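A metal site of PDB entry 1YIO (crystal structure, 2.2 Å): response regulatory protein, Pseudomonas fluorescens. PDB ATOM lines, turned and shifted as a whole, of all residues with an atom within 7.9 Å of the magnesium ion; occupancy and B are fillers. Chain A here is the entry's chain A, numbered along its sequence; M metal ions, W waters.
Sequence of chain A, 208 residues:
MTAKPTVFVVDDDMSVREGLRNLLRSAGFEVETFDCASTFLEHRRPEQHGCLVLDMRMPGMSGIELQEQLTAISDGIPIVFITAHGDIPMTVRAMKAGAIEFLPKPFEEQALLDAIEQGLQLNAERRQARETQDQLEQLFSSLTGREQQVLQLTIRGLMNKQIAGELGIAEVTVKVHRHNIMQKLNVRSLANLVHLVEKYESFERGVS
NZ of Lys 105 is in salt-bridge range of OD2 of Asp 11, at 2.8 Å. OD1 of Asp 11 is in hydrogen-bond range of N of Asp 13. N of Asp 55 sits at hydrogen-bond distance from O of Val 10 (2.9 Å). The side-chain carboxylate (OD1) of Asp 55 is in salt-bridge range of the side-chain amino group (NZ) of Lys 105. The guanidinium group (NH1) of Arg 57 lies within hydrogen-bond range of a ring nitrogen (NE2) of His 85, at 3.1 Å.
Asp 11 touches the magnesium ion (OD1 to MG, 3.9 Å). Of the 16 residues printed, 4 come within 4 Å of the magnesium ion. The nearest printed residue that does not touch the magnesium ion is Lys 105 (4.1 Å).
The magnesium ion is bound by water W1 (2.0 Å), the side-chain carboxylate (OD2) of Asp 55 (2.0 Å), water W2 (2.1 Å), the backbone carbonyl oxygen (O) of Arg 57 (2.1 Å), water W3 (2.2 Å) and the side-chain carboxylate (OD2) of Asp 12 (2.2 Å). The magnesium ion has six donor atoms within binding distance.
Water W1 bridges OD1 of Asp 55 (2.8 Å) and NZ of Lys 105 (3.5 Å). Water W2 lies within hydrogen-bond range of the side-chain carboxylate (OD1) of Asp 11 and the side-chain amino group (NZ) of Lys 105.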
ATOM      1  N   VAL A  10      12.992  -3.215   2.470  1.00  0.00           N
ATOM      2  CA  VAL A  10      13.724  -3.025   3.705  1.00  0.00           C
ATOM      3  C   VAL A  10      13.356  -1.685   4.322  1.00  0.00           C
ATOM      4  O   VAL A  10      13.715  -0.644   3.784  1.00  0.00           O
ATOM      5  CB  VAL A  10      15.232  -3.150   3.492  1.00  0.00           C
ATOM      6  CG1 VAL A  10      15.998  -2.980   4.830  1.00  0.00           C
ATOM      7  CG2 VAL A  10      15.539  -4.495   2.842  1.00  0.00           C
ATOM      8  N   ASP A  11      12.648  -1.740   5.449  1.00  0.00           N
ATOM      9  CA  ASP A  11      12.123  -0.561   6.141  1.00  0.00           C
ATOM     10  C   ASP A  11      11.724  -0.982   7.543  1.00  0.00           C
ATOM     11  O   ASP A  11      11.063  -1.993   7.711  1.00  0.00           O
ATOM     12  CB  ASP A  11      10.893  -0.025   5.395  1.00  0.00           C
ATOM     13  CG  ASP A  11      10.492   1.391   5.808  1.00  0.00           C
ATOM     14  OD1 ASP A  11      10.292   1.683   7.004  1.00  0.00           O
ATOM     15  OD2 ASP A  11      10.355   2.233   4.909  1.00  0.00           O
ATOM     16  N   ASP A  12      12.128  -0.216   8.564  1.00  0.00           N
ATOM     17  CA  ASP A  12      11.823  -0.566   9.962  1.00  0.00           C
ATOM     18  C   ASP A  12      10.326  -0.473  10.337  1.00  0.00           C
ATOM     19  O   ASP A  12       9.866  -1.087  11.318  1.00  0.00           O
ATOM     20  CB  ASP A  12      12.649   0.273  10.953  1.00  0.00           C
ATOM     21  CG  ASP A  12      12.680   1.761  10.579  1.00  0.00           C
ATOM     22  OD1 ASP A  12      12.281   2.591  11.419  1.00  0.00           O
ATOM     23  OD2 ASP A  12      13.077   2.115   9.441  1.00  0.00           O
ATOM     24  N   ASP A  13       9.563   0.288   9.562  1.00  0.00           N
ATOM     25  CA  ASP A  13       8.191   0.643   9.919  1.00  0.00           C
ATOM     26  C   ASP A  13       7.236  -0.433   9.436  1.00  0.00           C
ATOM     27  O   ASP A  13       7.238  -0.788   8.244  1.00  0.00           O
ATOM     28  CB  ASP A  13       7.839   2.010   9.316  1.00  0.00           C
ATOM     29  CG  ASP A  13       6.349   2.336   9.392  1.00  0.00           C
ATOM     30  OD1 ASP A  13       5.703   2.059  10.426  1.00  0.00           O
ATOM     31  OD2 ASP A  13       5.798   2.902   8.420  1.00  0.00           O
ATOM     32  N   VAL A  16       4.780   0.328   6.479  1.00  0.00           N
ATOM     33  CA  VAL A  16       5.437   0.278   5.178  1.00  0.00           C
ATOM     34  C   VAL A  16       5.618  -1.167   4.715  1.00  0.00           C
ATOM     35  O   VAL A  16       5.261  -1.499   3.584  1.00  0.00           O
ATOM     36  CB  VAL A  16       6.780   1.022   5.178  1.00  0.00           C
ATOM     37  CG1 VAL A  16       7.507   0.775   3.854  1.00  0.00           C
ATOM     38  CG2 VAL A  16       6.542   2.527   5.426  1.00  0.00           C
ATOM     39  N   ASP A  35      13.190  -5.656   8.597  1.00  0.00           N
ATOM     40  CA  ASP A  35      13.001  -4.392   9.325  1.00  0.00           C
ATOM     41  C   ASP A  35      14.363  -3.725   9.613  1.00  0.00           C
ATOM     42  O   ASP A  35      14.425  -2.644  10.221  1.00  0.00           O
ATOM     43  CB  ASP A  35      12.161  -4.633  10.592  1.00  0.00           C
ATOM     44  CG  ASP A  35      12.886  -5.464  11.656  1.00  0.00           C
ATOM     45  OD1 ASP A  35      12.407  -5.529  12.809  1.00  0.00           O
ATOM     46  OD2 ASP A  35      13.956  -6.035  11.337  1.00  0.00           O
ATOM     47  N   ASP A  55      14.397   1.909   2.570  1.00  0.00           N
ATOM     48  CA  ASP A  55      14.263   3.026   3.456  1.00  0.00           C
ATOM     49  C   ASP A  55      15.643   3.678   3.699  1.00  0.00           C
ATOM     50  O   ASP A  55      16.649   2.974   3.815  1.00  0.00           O
ATOM     51  CB  ASP A  55      13.721   2.493   4.784  1.00  0.00           C
ATOM     52  CG  ASP A  55      13.281   3.591   5.733  1.00  0.00           C
ATOM     53  OD1 ASP A  55      13.077   4.746   5.291  1.00  0.00           O
ATOM     54  OD2 ASP A  55      13.122   3.302   6.926  1.00  0.00           O
ATOM     55  N   MET A  56      15.679   5.012   3.768  1.00  0.00           N
ATOM     56  CA  MET A  56      16.891   5.759   4.111  1.00  0.00           C
ATOM     57  C   MET A  56      17.321   5.588   5.556  1.00  0.00           C
ATOM     58  O   MET A  56      18.515   5.387   5.826  1.00  0.00           O
ATOM     59  CB  MET A  56      16.754   7.263   3.791  1.00  0.00           C
ATOM     60  CG  MET A  56      16.575   7.567   2.281  1.00  0.00           C
ATOM     61  SD  MET A  56      18.064   7.452   1.258  1.00  0.00           S
ATOM     62  CE  MET A  56      18.660   5.830   1.644  1.00  0.00           C
ATOM     63  N   ARG A  57      16.379   5.709   6.479  1.00  0.00           N
ATOM     64  CA  ARG A  57      16.705   5.665   7.916  1.00  0.00           C
ATOM     65  C   ARG A  57      16.097   4.490   8.647  1.00  0.00           C
ATOM     66  O   ARG A  57      14.876   4.321   8.662  1.00  0.00           O
ATOM     67  CB  ARG A  57      16.233   6.974   8.607  1.00  0.00           C
ATOM     68  CG  ARG A  57      16.646   8.302   7.986  1.00  0.00           C
ATOM     69  CD  ARG A  57      16.005   9.496   8.681  1.00  0.00           C
ATOM     70  NE  ARG A  57      16.147  10.741   7.933  1.00  0.00           N
ATOM     71  CZ  ARG A  57      15.919  11.966   8.414  1.00  0.00           C
ATOM     72  NH1 ARG A  57      15.519  12.110   9.671  1.00  0.00           N
ATOM     73  NH2 ARG A  57      16.096  13.028   7.645  1.00  0.00           N
ATOM     74  N   MET A  58      16.953   3.676   9.262  1.00  0.00           N
ATOM     75  CA  MET A  58      16.505   2.483   9.970  1.00  0.00           C
ATOM     76  C   MET A  58      17.471   2.267  11.121  1.00  0.00           C
ATOM     77  O   MET A  58      18.536   2.859  11.105  1.00  0.00           O
ATOM     78  CB  MET A  58      16.569   1.261   9.050  1.00  0.00           C
ATOM     79  CG  MET A  58      15.802   1.370   7.761  1.00  0.00           C
ATOM     80  SD  MET A  58      16.050  -0.142   6.814  1.00  0.00           S
ATOM     81  CE  MET A  58      17.603   0.268   6.036  1.00  0.00           C
ATOM     82  N   PRO A  59      17.092   1.457  12.132  1.00  0.00           N
ATOM     83  CA  PRO A  59      18.049   1.081  13.175  1.00  0.00           C
ATOM     84  C   PRO A  59      19.275   0.378  12.605  1.00  0.00           C
ATOM     85  O   PRO A  59      19.151  -0.530  11.774  1.00  0.00           O
ATOM     86  CB  PRO A  59      17.235   0.122  14.059  1.00  0.00           C
ATOM     87  CG  PRO A  59      15.784   0.611  13.889  1.00  0.00           C
ATOM     88  CD  PRO A  59      15.747   0.897  12.403  1.00  0.00           C
ATOM     89  N   ILE A  82      13.341   4.991  -0.736  1.00  0.00           N
ATOM     90  CA  ILE A  82      12.130   5.662  -0.233  1.00  0.00           C
ATOM     91  C   ILE A  82      12.497   6.409   1.036  1.00  0.00           C
ATOM     92  O   ILE A  82      13.401   5.985   1.768  1.00  0.00           O
ATOM     93  CB  ILE A  82      10.949   4.670   0.011  1.00  0.00           C
ATOM     94  CG1 ILE A  82      11.353   3.527   0.956  1.00  0.00           C
ATOM     95  CG2 ILE A  82      10.465   4.083  -1.336  1.00  0.00           C
ATOM     96  CD1 ILE A  82      10.177   2.750   1.528  1.00  0.00           C
ATOM     97  N   THR A  83      11.857   7.541   1.279  1.00  0.00           N
ATOM     98  CA  THR A  83      12.228   8.310   2.465  1.00  0.00           C
ATOM     99  C   THR A  83      11.063   9.163   2.943  1.00  0.00           C
ATOM    100  O   THR A  83      10.252   9.621   2.153  1.00  0.00           O
ATOM    101  CB  THR A  83      13.461   9.218   2.182  1.00  0.00           C
ATOM    102  OG1 THR A  83      13.853   9.888   3.373  1.00  0.00           O
ATOM    103  CG2 THR A  83      13.171  10.272   1.130  1.00  0.00           C
ATOM    104  N   ALA A  84      11.008   9.379   4.254  1.00  0.00           N
ATOM    105  CA  ALA A  84      10.076  10.347   4.821  1.00  0.00           C
ATOM    106  C   ALA A  84      10.663  11.778   4.871  1.00  0.00           C
ATOM    107  O   ALA A  84       9.959  12.709   5.248  1.00  0.00           O
ATOM    108  CB  ALA A  84       9.635   9.896   6.216  1.00  0.00           C
ATOM    109  N   HIS A  85      11.931  11.928   4.493  1.00  0.00           N
ATOM    110  CA  HIS A  85      12.616  13.238   4.501  1.00  0.00           C
ATOM    111  C   HIS A  85      13.111  13.650   3.131  1.00  0.00           C
ATOM    112  O   HIS A  85      14.325  13.665   2.859  1.00  0.00           O
ATOM    113  CB  HIS A  85      13.757  13.238   5.520  1.00  0.00           C
ATOM    114  CG  HIS A  85      13.325  12.720   6.849  1.00  0.00           C
ATOM    115  ND1 HIS A  85      13.173  11.370   7.099  1.00  0.00           N
ATOM    116  CD2 HIS A  85      12.925  13.358   7.972  1.00  0.00           C
ATOM    117  CE1 HIS A  85      12.730  11.201   8.322  1.00  0.00           C
ATOM    118  NE2 HIS A  85      12.567  12.389   8.881  1.00  0.00           N
ATOM    119  N   LYS A 105       7.864   8.943   1.143  1.00  0.00           N
ATOM    120  CA  LYS A 105       6.833   8.281   1.906  1.00  0.00           C
ATOM    121  C   LYS A 105       6.000   9.410   2.457  1.00  0.00           C
ATOM    122  O   LYS A 105       6.561  10.362   2.971  1.00  0.00           O
ATOM    123  CB  LYS A 105       7.440   7.479   3.062  1.00  0.00           C
ATOM    124  CG  LYS A 105       8.069   6.155   2.646  1.00  0.00           C
ATOM    125  CD  LYS A 105       8.501   5.311   3.850  1.00  0.00           C
ATOM    126  CE  LYS A 105       9.876   5.674   4.354  1.00  0.00           C
ATOM    127  NZ  LYS A 105      10.182   4.945   5.608  1.00  0.00           N
HETATM  128 MG    MG M   1      12.754   4.215   8.718  1.00  0.00          MG
HETATM  129  O   HOH W   1      12.655   6.013   7.808  1.00  0.00           O
HETATM  130  O   HOH W   2      10.731   3.819   8.238  1.00  0.00           O
HETATM  131  O   HOH W   3      12.532   4.874  10.815  1.00  0.00           O
